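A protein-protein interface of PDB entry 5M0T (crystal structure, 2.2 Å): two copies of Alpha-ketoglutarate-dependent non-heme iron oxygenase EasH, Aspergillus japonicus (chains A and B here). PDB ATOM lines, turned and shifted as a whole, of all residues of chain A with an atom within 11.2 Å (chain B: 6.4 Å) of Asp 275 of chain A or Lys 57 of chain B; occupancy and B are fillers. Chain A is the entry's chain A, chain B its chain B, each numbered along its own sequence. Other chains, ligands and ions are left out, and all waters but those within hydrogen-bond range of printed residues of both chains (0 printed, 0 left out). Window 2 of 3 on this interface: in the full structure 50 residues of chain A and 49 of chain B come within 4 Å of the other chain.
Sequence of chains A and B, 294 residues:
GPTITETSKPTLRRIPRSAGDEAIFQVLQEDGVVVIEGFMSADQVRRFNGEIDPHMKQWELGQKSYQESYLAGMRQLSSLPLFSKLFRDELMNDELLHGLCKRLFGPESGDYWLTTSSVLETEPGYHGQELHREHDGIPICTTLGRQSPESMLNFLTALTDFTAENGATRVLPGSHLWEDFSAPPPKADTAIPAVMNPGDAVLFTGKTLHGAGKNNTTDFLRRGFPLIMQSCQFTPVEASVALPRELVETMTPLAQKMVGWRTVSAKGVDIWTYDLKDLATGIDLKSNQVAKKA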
ATOM      1  N   THR A 263      18.588 -20.649  36.292  1.00  0.00           N
ATOM      2  CA  THR A 263      17.192 -20.285  36.250  1.00  0.00           C
ATOM      3  C   THR A 263      16.370 -21.394  36.898  1.00  0.00           C
ATOM      4  O   THR A 263      16.667 -22.575  36.745  1.00  0.00           O
ATOM      5  CB  THR A 263      16.773 -20.015  34.797  1.00  0.00           C
ATOM      6  OG1 THR A 263      17.435 -18.826  34.341  1.00  0.00           O
ATOM      7  CG2 THR A 263      15.244 -19.881  34.627  1.00  0.00           C
ATOM      8  N   ASP A 270       9.610 -18.764  34.676  1.00  0.00           N
ATOM      9  CA  ASP A 270      11.057 -18.748  34.785  1.00  0.00           C
ATOM     10  C   ASP A 270      11.450 -17.518  35.564  1.00  0.00           C
ATOM     11  O   ASP A 270      11.065 -16.421  35.193  1.00  0.00           O
ATOM     12  CB  ASP A 270      11.749 -18.739  33.411  1.00  0.00           C
ATOM     13  CG  ASP A 270      11.807 -20.123  32.769  1.00  0.00           C
ATOM     14  OD1 ASP A 270      11.465 -21.119  33.431  1.00  0.00           O
ATOM     15  OD2 ASP A 270      12.201 -20.215  31.593  1.00  0.00           O
ATOM     16  N   ILE A 271      12.197 -17.714  36.647  1.00  0.00           N
ATOM     17  CA  ILE A 271      12.758 -16.611  37.414  1.00  0.00           C
ATOM     18  C   ILE A 271      14.248 -16.850  37.664  1.00  0.00           C
ATOM     19  O   ILE A 271      14.742 -17.969  37.476  1.00  0.00           O
ATOM     20  CB  ILE A 271      11.976 -16.366  38.735  1.00  0.00           C
ATOM     21  CG1 ILE A 271      12.079 -17.546  39.699  1.00  0.00           C
ATOM     22  CG2 ILE A 271      10.511 -16.066  38.432  1.00  0.00           C
ATOM     23  CD1 ILE A 271      11.344 -17.299  40.998  1.00  0.00           C
ATOM     24  N   TRP A 272      14.943 -15.784  38.077  1.00  0.00           N
ATOM     25  CA  TRP A 272      16.403 -15.764  38.160  1.00  0.00           C
ATOM     26  C   TRP A 272      17.000 -15.982  36.753  1.00  0.00           C
ATOM     27  O   TRP A 272      17.726 -16.934  36.487  1.00  0.00           O
ATOM     28  CB  TRP A 272      16.901 -16.786  39.184  1.00  0.00           C
ATOM     29  CG  TRP A 272      18.157 -16.403  39.880  1.00  0.00           C
ATOM     30  CD1 TRP A 272      19.345 -17.070  39.858  1.00  0.00           C
ATOM     31  CD2 TRP A 272      18.346 -15.274  40.751  1.00  0.00           C
ATOM     32  NE1 TRP A 272      20.268 -16.424  40.656  1.00  0.00           N
ATOM     33  CE2 TRP A 272      19.674 -15.326  41.223  1.00  0.00           C
ATOM     34  CE3 TRP A 272      17.510 -14.241  41.199  1.00  0.00           C
ATOM     35  CZ2 TRP A 272      20.200 -14.359  42.081  1.00  0.00           C
ATOM     36  CZ3 TRP A 272      18.035 -13.290  42.065  1.00  0.00           C
ATOM     37  CH2 TRP A 272      19.366 -13.358  42.499  1.00  0.00           C
ATOM     38  N   THR A 273      16.683 -15.043  35.876  1.00  0.00           N
ATOM     39  CA  THR A 273      17.019 -15.105  34.474  1.00  0.00           C
ATOM     40  C   THR A 273      18.053 -14.052  34.078  1.00  0.00           C
ATOM     41  O   THR A 273      18.354 -13.139  34.845  1.00  0.00           O
ATOM     42  CB  THR A 273      15.745 -14.851  33.671  1.00  0.00           C
ATOM     43  OG1 THR A 273      15.298 -13.521  33.921  1.00  0.00           O
ATOM     44  CG2 THR A 273      14.640 -15.842  34.082  1.00  0.00           C
ATOM     45  N   TYR A 274      18.619 -14.219  32.883  1.00  0.00           N
ATOM     46  CA  TYR A 274      19.376 -13.174  32.199  1.00  0.00           C
ATOM     47  C   TYR A 274      18.529 -12.724  31.034  1.00  0.00           C
ATOM     48  O   TYR A 274      18.200 -13.530  30.163  1.00  0.00           O
ATOM     49  CB  TYR A 274      20.709 -13.692  31.675  1.00  0.00           C
ATOM     50  CG  TYR A 274      21.431 -12.678  30.819  1.00  0.00           C
ATOM     51  CD1 TYR A 274      22.010 -11.572  31.390  1.00  0.00           C
ATOM     52  CD2 TYR A 274      21.501 -12.810  29.438  1.00  0.00           C
ATOM     53  CE1 TYR A 274      22.685 -10.631  30.621  1.00  0.00           C
ATOM     54  CE2 TYR A 274      22.150 -11.871  28.654  1.00  0.00           C
ATOM     55  CZ  TYR A 274      22.751 -10.785  29.255  1.00  0.00           C
ATOM     56  OH  TYR A 274      23.409  -9.845  28.496  1.00  0.00           O
ATOM     57  N   ASP A 275      18.170 -11.449  31.026  1.00  0.00           N
ATOM     58  CA  ASP A 275      17.325 -10.870  29.995  1.00  0.00           C
ATOM     59  C   ASP A 275      15.974 -11.597  29.831  1.00  0.00           C
ATOM     60  O   ASP A 275      15.443 -11.681  28.723  1.00  0.00           O
ATOM     61  CB  ASP A 275      18.110 -10.862  28.671  1.00  0.00           C
ATOM     62  CG  ASP A 275      17.587  -9.855  27.674  1.00  0.00           C
ATOM     63  OD1 ASP A 275      16.736  -9.002  28.021  1.00  0.00           O
ATOM     64  OD2 ASP A 275      18.047  -9.925  26.521  1.00  0.00           O
ATOM     65  N   LEU A 276      15.444 -12.132  30.934  1.00  0.00           N
ATOM     66  CA  LEU A 276      14.220 -12.960  30.937  1.00  0.00           C
ATOM     67  C   LEU A 276      14.349 -14.361  30.288  1.00  0.00           C
ATOM     68  O   LEU A 276      13.393 -15.132  30.302  1.00  0.00           O
ATOM     69  CB  LEU A 276      13.040 -12.192  30.322  1.00  0.00           C
ATOM     70  CG  LEU A 276      12.766 -10.802  30.907  1.00  0.00           C
ATOM     71  CD1 LEU A 276      11.660 -10.111  30.134  1.00  0.00           C
ATOM     72  CD2 LEU A 276      12.386 -10.888  32.386  1.00  0.00           C
ATOM     73  N   LYS A 277      15.523 -14.683  29.755  1.00  0.00           N
ATOM     74  CA  LYS A 277      15.808 -15.979  29.143  1.00  0.00           C
ATOM     75  C   LYS A 277      16.710 -16.740  30.129  1.00  0.00           C
ATOM     76  O   LYS A 277      17.075 -16.204  31.183  1.00  0.00           O
ATOM     77  CB  LYS A 277      16.506 -15.810  27.762  1.00  0.00           C
ATOM     78  CG  LYS A 277      16.004 -14.717  26.798  1.00  0.00           C
ATOM     79  CD  LYS A 277      15.036 -15.208  25.728  1.00  0.00           C
ATOM     80  N   ASP A 278      17.058 -17.979  29.782  1.00  0.00           N
ATOM     81  CA  ASP A 278      17.876 -18.879  30.614  1.00  0.00           C
ATOM     82  C   ASP A 278      19.195 -18.219  31.065  1.00  0.00           C
ATOM     83  O   ASP A 278      19.895 -17.608  30.260  1.00  0.00           O
ATOM     84  CB  ASP A 278      18.170 -20.166  29.826  1.00  0.00           C
ATOM     85  CG  ASP A 278      18.897 -21.210  30.649  1.00  0.00           C
ATOM     86  OD1 ASP A 278      18.281 -21.713  31.609  1.00  0.00           O
ATOM     87  OD2 ASP A 278      20.067 -21.541  30.329  1.00  0.00           O
ATOM     88  N   LEU A 279      19.513 -18.343  32.352  1.00  0.00           N
ATOM     89  CA  LEU A 279      20.664 -17.631  32.949  1.00  0.00           C
ATOM     90  C   LEU A 279      21.998 -18.207  32.485  1.00  0.00           C
ATOM     91  O   LEU A 279      22.891 -17.471  32.052  1.00  0.00           O
ATOM     92  CB  LEU A 279      20.595 -17.675  34.483  1.00  0.00           C
ATOM     93  CG  LEU A 279      21.781 -17.082  35.279  1.00  0.00           C
ATOM     94  CD1 LEU A 279      22.068 -15.641  34.878  1.00  0.00           C
ATOM     95  CD2 LEU A 279      21.520 -17.212  36.784  1.00  0.00           C
ATOM     96  N   ALA A 280      22.118 -19.525  32.601  1.00  0.00           N
ATOM     97  CA  ALA A 280      23.340 -20.243  32.224  1.00  0.00           C
ATOM     98  C   ALA A 280      23.743 -20.039  30.759  1.00  0.00           C
ATOM     99  O   ALA A 280      24.928 -19.909  30.463  1.00  0.00           O
ATOM    100  CB  ALA A 280      23.179 -21.726  32.524  1.00  0.00           C
ATOM    101  N   THR A 281      22.758 -20.012  29.858  1.00  0.00           N
ATOM    102  CA  THR A 281      22.988 -19.731  28.437  1.00  0.00           C
ATOM    103  C   THR A 281      23.476 -18.300  28.248  1.00  0.00           C
ATOM    104  O   THR A 281      24.433 -18.059  27.504  1.00  0.00           O
ATOM    105  CB  THR A 281      21.695 -19.893  27.584  1.00  0.00           C
ATOM    106  OG1 THR A 281      21.060 -21.141  27.879  1.00  0.00           O
ATOM    107  CG2 THR A 281      21.990 -19.830  26.097  1.00  0.00           C
ATOM    108  N   GLY A 282      22.807 -17.360  28.911  1.00  0.00           N
ATOM    109  CA  GLY A 282      23.058 -15.940  28.718  1.00  0.00           C
ATOM    110  C   GLY A 282      24.429 -15.482  29.154  1.00  0.00           C
ATOM    111  O   GLY A 282      25.024 -14.627  28.508  1.00  0.00           O
ATOM    112  N   ILE A 283      24.926 -16.057  30.249  1.00  0.00           N
ATOM    113  CA  ILE A 283      26.260 -15.739  30.785  1.00  0.00           C
ATOM    114  C   ILE A 283      27.348 -16.733  30.352  1.00  0.00           C
ATOM    115  O   ILE A 283      28.494 -16.571  30.752  1.00  0.00           O
ATOM    116  CB  ILE A 283      26.258 -15.585  32.332  1.00  0.00           C
ATOM    117  CG1 ILE A 283      26.052 -16.928  33.055  1.00  0.00           C
ATOM    118  CG2 ILE A 283      25.205 -14.570  32.754  1.00  0.00           C
ATOM    119  CD1 ILE A 283      25.961 -16.826  34.566  1.00  0.00           C
ATOM    120  N   ASP A 284      26.979 -17.744  29.555  1.00  0.00           N
ATOM    121  CA  ASP A 284      27.904 -18.756  28.998  1.00  0.00           C
ATOM    122  C   ASP A 284      28.502 -19.648  30.092  1.00  0.00           C
ATOM    123  O   ASP A 284      29.674 -20.006  30.037  1.00  0.00           O
ATOM    124  CB  ASP A 284      28.999 -18.092  28.141  1.00  0.00           C
ATOM    125  N   HIS B  55      20.925  -1.845  21.744  1.00  0.00           N
ATOM    126  CA  HIS B  55      20.861  -3.213  22.313  1.00  0.00           C
ATOM    127  C   HIS B  55      19.528  -3.966  22.105  1.00  0.00           C
ATOM    128  O   HIS B  55      19.414  -5.119  22.524  1.00  0.00           O
ATOM    129  CB  HIS B  55      21.184  -3.170  23.816  1.00  0.00           C
ATOM    130  CG  HIS B  55      22.520  -2.557  24.130  1.00  0.00           C
ATOM    131  ND1 HIS B  55      23.678  -3.304  24.222  1.00  0.00           N
ATOM    132  CD2 HIS B  55      22.879  -1.279  24.408  1.00  0.00           C
ATOM    133  CE1 HIS B  55      24.688  -2.517  24.545  1.00  0.00           C
ATOM    134  NE2 HIS B  55      24.233  -1.283  24.662  1.00  0.00           N
ATOM    135  N   MET B  56      18.536  -3.341  21.462  1.00  0.00           N
ATOM    136  CA  MET B  56      17.184  -3.934  21.325  1.00  0.00           C
ATOM    137  C   MET B  56      17.153  -5.111  20.334  1.00  0.00           C
ATOM    138  O   MET B  56      17.900  -5.121  19.345  1.00  0.00           O
ATOM    139  CB  MET B  56      16.140  -2.875  20.886  1.00  0.00           C
ATOM    140  CG  MET B  56      15.858  -1.760  21.891  1.00  0.00           C
ATOM    141  SD  MET B  56      15.006  -2.317  23.384  1.00  0.00           S
ATOM    142  CE  MET B  56      13.333  -2.482  22.783  1.00  0.00           C
ATOM    143  N   LYS B  57      16.289  -6.095  20.612  1.00  0.00           N
ATOM    144  CA  LYS B  57      16.036  -7.212  19.680  1.00  0.00           C
ATOM    145  C   LYS B  57      14.709  -7.947  19.962  1.00  0.00           C
ATOM    146  O   LYS B  57      14.029  -7.692  20.968  1.00  0.00           O
ATOM    147  CB  LYS B  57      17.236  -8.191  19.636  1.00  0.00           C
ATOM    148  CG  LYS B  57      17.296  -9.276  20.705  1.00  0.00           C
ATOM    149  CD  LYS B  57      17.285  -8.702  22.106  1.00  0.00           C
ATOM    150  CE  LYS B  57      17.523  -9.767  23.157  1.00  0.00           C
ATOM    151  NZ  LYS B  57      16.670  -9.537  24.354  1.00  0.00           N
ATOM    152  N   GLN B  58      14.354  -8.858  19.056  1.00  0.00           N
ATOM    153  CA  GLN B  58      13.106  -9.626  19.150  1.00  0.00           C
ATOM    154  C   GLN B  58      13.186 -10.681  20.270  1.00  0.00           C
ATOM    155  O   GLN B  58      14.269 -11.192  20.572  1.00  0.00           O
ATOM    156  CB  GLN B  58      12.808 -10.294  17.794  1.00  0.00           C
ATOM    157  CG  GLN B  58      11.414 -10.899  17.638  1.00  0.00           C
ATOM    158  CD  GLN B  58      10.281  -9.879  17.695  1.00  0.00           C
ATOM    159  OE1 GLN B  58      10.483  -8.685  17.464  1.00  0.00           O
ATOM    160  NE2 GLN B  58       9.075 -10.353  18.000  1.00  0.00           N
ATOM    161  N   TRP B  59      12.045 -10.985  20.892  1.00  0.00           N
ATOM    162  CA  TRP B  59      11.948 -12.094  21.850  1.00  0.00           C
ATOM    163  C   TRP B  59      12.160 -13.447  21.143  1.00  0.00           C
ATOM    164  O   TRP B  59      11.432 -13.768  20.192  1.00  0.00           O
ATOM    165  CB  TRP B  59      10.589 -12.091  22.564  1.00  0.00           C
ATOM    166  CG  TRP B  59      10.372 -13.292  23.461  1.00  0.00           C
ATOM    167  CD1 TRP B  59       9.805 -14.494  23.113  1.00  0.00           C
ATOM    168  CD2 TRP B  59      10.735 -13.410  24.841  1.00  0.00           C
ATOM    169  NE1 TRP B  59       9.794 -15.346  24.194  1.00  0.00           N
ATOM    170  CE2 TRP B  59      10.358 -14.706  25.269  1.00  0.00           C
ATOM    171  CE3 TRP B  59      11.334 -12.544  25.763  1.00  0.00           C
ATOM    172  CZ2 TRP B  59      10.561 -15.150  26.584  1.00  0.00           C
ATOM    173  CZ3 TRP B  59      11.536 -12.991  27.066  1.00  0.00           C
ATOM    174  CH2 TRP B  59      11.147 -14.281  27.463  1.00  0.00           C
ATOM    175  N   MET B  74       6.828  -9.107  20.960  1.00  0.00           N
ATOM    176  CA  MET B  74       7.374  -7.816  21.392  1.00  0.00           C
ATOM    177  C   MET B  74       8.862  -7.753  21.123  1.00  0.00           C
ATOM    178  O   MET B  74       9.537  -8.795  21.096  1.00  0.00           O
ATOM    179  CB  MET B  74       7.151  -7.616  22.891  1.00  0.00           C
ATOM    180  CG  MET B  74       5.709  -7.381  23.277  1.00  0.00           C
ATOM    181  SD  MET B  74       5.603  -7.038  25.045  1.00  0.00           S
ATOM    182  CE  MET B  74       4.243  -5.871  25.094  1.00  0.00           C
ATOM    183  N   ARG B  75       9.363  -6.535  20.922  1.00  0.00           N
ATOM    184  CA  ARG B  75      10.791  -6.250  21.079  1.00  0.00           C
ATOM    185  C   ARG B  75      11.024  -5.973  22.566  1.00  0.00           C
ATOM    186  O   ARG B  75      10.278  -5.206  23.179  1.00  0.00           O
ATOM    187  CB  ARG B  75      11.215  -5.052  20.228  1.00  0.00           C
ATOM    188  CG  ARG B  75      10.980  -5.241  18.737  1.00  0.00           C
ATOM    189  CD  ARG B  75      11.574  -4.108  17.920  1.00  0.00           C
ATOM    190  NE  ARG B  75      13.031  -4.035  18.055  1.00  0.00           N
ATOM    191  CZ  ARG B  75      13.920  -4.727  17.338  1.00  0.00           C
ATOM    192  NH1 ARG B  75      13.548  -5.594  16.389  1.00  0.00           N
ATOM    193  NH2 ARG B  75      15.219  -4.546  17.572  1.00  0.00           N
ATOM    194  N   GLN B  76      12.021  -6.630  23.156  1.00  0.00           N
ATOM    195  CA  GLN B  76      12.312  -6.455  24.572  1.00  0.00           C
ATOM    196  C   GLN B  76      13.808  -6.499  24.882  1.00  0.00           C
ATOM    197  O   GLN B  76      14.577  -7.241  24.261  1.00  0.00           O
ATOM    198  CB  GLN B  76      11.525  -7.457  25.454  1.00  0.00           C
ATOM    199  CG  GLN B  76      11.959  -8.931  25.398  1.00  0.00           C
ATOM    200  CD  GLN B  76      13.106  -9.314  26.352  1.00  0.00           C
ATOM    201  OE1 GLN B  76      13.319  -8.689  27.392  1.00  0.00           O
ATOM    202  NE2 GLN B  76      13.849 -10.360  25.986  1.00  0.00           N
ATOM    203  N   LEU B  77      14.193  -5.661  25.839  1.00  0.00           N
ATOM    204  CA  LEU B  77      15.502  -5.697  26.470  1.00  0.00           C
ATOM    205  C   LEU B  77      15.261  -5.648  27.968  1.00  0.00           C
ATOM    206  O   LEU B  77      14.517  -4.802  28.433  1.00  0.00           O
ATOM    207  CB  LEU B  77      16.325  -4.482  26.047  1.00  0.00           C
ATOM    208  CG  LEU B  77      17.745  -4.395  26.617  1.00  0.00           C
ATOM    209  CD1 LEU B  77      18.625  -5.518  26.083  1.00  0.00           C
ATOM    210  CD2 LEU B  77      18.367  -3.038  26.297  1.00  0.00           C
ATOM    211  N   SER B  78      15.890  -6.550  28.708  1.00  0.00           N
ATOM    212  CA  SER B  78      15.780  -6.599  30.166  1.00  0.00           C
ATOM    213  C   SER B  78      17.184  -6.617  30.779  1.00  0.00           C
ATOM    214  O   SER B  78      18.154  -6.368  30.067  1.00  0.00           O
ATOM    215  CB  SER B  78      14.941  -7.807  30.576  1.00  0.00           C
ATOM    216  OG  SER B  78      13.645  -7.693  30.020  1.00  0.00           O
ATOM    217  N   SER B  79      17.308  -6.857  32.078  1.00  0.00           N
ATOM    218  CA  SER B  79      18.597  -6.698  32.773  1.00  0.00           C
ATOM    219  C   SER B  79      19.271  -5.352  32.387  1.00  0.00           C
ATOM    220  O   SER B  79      20.421  -5.306  31.930  1.00  0.00           O
ATOM    221  CB  SER B  79      19.498  -7.904  32.502  1.00  0.00           C
ATOM    222  OG  SER B  79      18.825  -9.113  32.843  1.00  0.00           O
ATOM    223  N   PHE B  83      22.976  -2.259  30.803  1.00  0.00           N
ATOM    224  CA  PHE B  83      22.966  -1.455  29.582  1.00  0.00           C
ATOM    225  C   PHE B  83      22.791   0.052  29.758  1.00  0.00           C
ATOM    226  O   PHE B  83      23.022   0.785  28.799  1.00  0.00           O
ATOM    227  CB  PHE B  83      21.850  -1.986  28.653  1.00  0.00           C
ATOM    228  CG  PHE B  83      21.952  -3.463  28.382  1.00  0.00           C
ATOM    229  CD1 PHE B  83      22.969  -3.960  27.555  1.00  0.00           C
ATOM    230  CD2 PHE B  83      21.072  -4.365  28.987  1.00  0.00           C
ATOM    231  CE1 PHE B  83      23.083  -5.328  27.324  1.00  0.00           C
ATOM    232  CE2 PHE B  83      21.179  -5.733  28.752  1.00  0.00           C
ATOM    233  CZ  PHE B  83      22.192  -6.216  27.924  1.00  0.00           C
ATOM    234  N   GLU B 238      14.842 -11.194  37.431  1.00  0.00           N
ATOM    235  CA  GLU B 238      16.178 -10.964  36.874  1.00  0.00           C
ATOM    236  C   GLU B 238      17.264 -11.254  37.888  1.00  0.00           C
ATOM    237  O   GLU B 238      17.260 -10.677  38.976  1.00  0.00           O
ATOM    238  CB  GLU B 238      16.308  -9.525  36.414  1.00  0.00           C
ATOM    239  CG  GLU B 238      15.447  -9.222  35.207  1.00  0.00           C
ATOM    240  CD  GLU B 238      15.462  -7.758  34.823  1.00  0.00           C
ATOM    241  OE1 GLU B 238      16.287  -6.974  35.376  1.00  0.00           O
ATOM    242  OE2 GLU B 238      14.630  -7.388  33.956  1.00  0.00           O
ATOM    243  N   ALA B 242      24.118 -12.094  37.106  1.00  0.00           N
ATOM    244  CA  ALA B 242      24.478 -11.654  35.751  1.00  0.00           C
ATOM    245  C   ALA B 242      25.302 -10.369  35.719  1.00  0.00           C
ATOM    246  O   ALA B 242      25.996 -10.112  34.742  1.00  0.00           O
ATOM    247  CB  ALA B 242      23.227 -11.488  34.898  1.00  0.00           C
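No position is printed for both chains.
The side-chain amino group of Lys 57 of chain B is in salt-bridge range of the side-chain carboxylate of Asp 275 of chain A (2.6 Å). The side-chain amide nitrogen (NE2) of Gln 76 of chain B is in hydrogen-bond range of the backbone carbonyl oxygen (O) of Asp 275 of chain A (3.4 Å). The side-chain carboxylate of Asp 275 of chain A is in hydrogen-bond range of the backbone NH of Ser 78 of chain B (2.7 Å). The backbone NH of Asp 275 of chain A lies within hydrogen-bond range of the side-chain hydroxyl of Ser 79 of chain B.
Of the 16 printed residues of chain A, 4 touch a printed residue of chain B. Printed residues of chain A that touch a printed residue of chain B: Thr 273, Tyr 274, Asp 275 and Leu 276. Hydrophobic or aromatic side chains of chain A within 4 Å of the printed part of chain B: Tyr 274 and Leu 276. Hydrophobic or aromatic side chains of chain B that line the printed part of chain A: Trp 59, Phe 83 and Ala 242. Along chain B the printed residues that touch a printed residue of chain A span positions 57 to 242. Among the printed residues, 11 pairs touch across the chains. Among the printed residues, Asp or Glu carboxylates within 4 Å of a Lys or Arg side-chain nitrogen of the other chain: Asp 275 of chain A with Lys 57 of chain B (2.6 Å).
Among the printed residues, merely in contact across the chains: Thr 273 of chain A with Glu 238 of chain B (3.7 Å), Tyr 274 of chain A with Phe 83 of chain B (3.9 Å), Tyr 274 of chain A with Ala 242 of chain B (3.7 Å), Asp 275 of chain A with Leu 77 of chain B (3.7 Å), Leu 276 of chain A with Trp 59 of chain B (3.7 Å), Leu 276 of chain A with Gln 76 of chain B (3.5 Å) and Leu 276 of chain A with Ser 78 of chain B (3.1 Å).
The side-chain hydroxyl (OG1) of Thr 273 of chain A lies close to the backbone NH (N) of Leu 276 of chain A (3.3 Å). O of Gln 76 of chain B sits at hydrogen-bond distance from NZ of Lys 57 of chain B, 3.1 Å away. The backbone NH (N) of Trp 59 of chain B sits at hydrogen-bond distance from the backbone carbonyl oxygen (O) of Met 74 of chain B, 3.3 Å away. OG of Ser 78 of chain B sits at hydrogen-bond distance from OE1 of Gln 76 of chain B (2.8 Å). N of Ser 79 of chain B lies within hydrogen-bond range of OE2 of Glu 238 of chain B (3.3 Å).
Asp 275 of chain A touches just these residues of chain B: Lys 57, Gln 76, Leu 77, Ser 78 and Ser 79. Of chain A, only Asp 275 comes within 4 Å of Lys 57 of chain B. No residue of chain A comes within 4 Å of Gln 58 of chain B. No residue of chain A comes within 4 Å of Arg 75 of chain B. Of chain A, only Asp 275 (3.4 Å) and Leu 276 (3.5 Å) come within 4 Å of Gln 76 of chain B. Leu 77 of chain B touches just one residue of chain A: Asp 275 (3.7 Å). Ser 78 of chain B touches just these residues of chain A: Asp 275 (2.7 Å) and Leu 276 (3.1 Å). Ser 79 of chain B touches just one residue of chain A: Asp 275. Printed residues of chain B within 4 Å of Tyr 274 of chain A: Phe 83 and Ala 242. Printed residues of chain B within 4 Å of Leu 276 of chain A: Trp 59 (3.7 Å), Gln 76 (3.5 Å) and Ser 78 (3.1 Å). Of the printed residues of chain B, Thr 273 of chain A touches Glu 238. Printed residues of chain A within 4 Å of Trp 59 of chain B: Leu 276. Printed residues of chain A within 4 Å of Phe 83 of chain B: Tyr 274 (3.9 Å). The nearest printed residue of chain A that does not touch Glu 238 of chain B is Trp 272 of chain A (4.1 Å).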
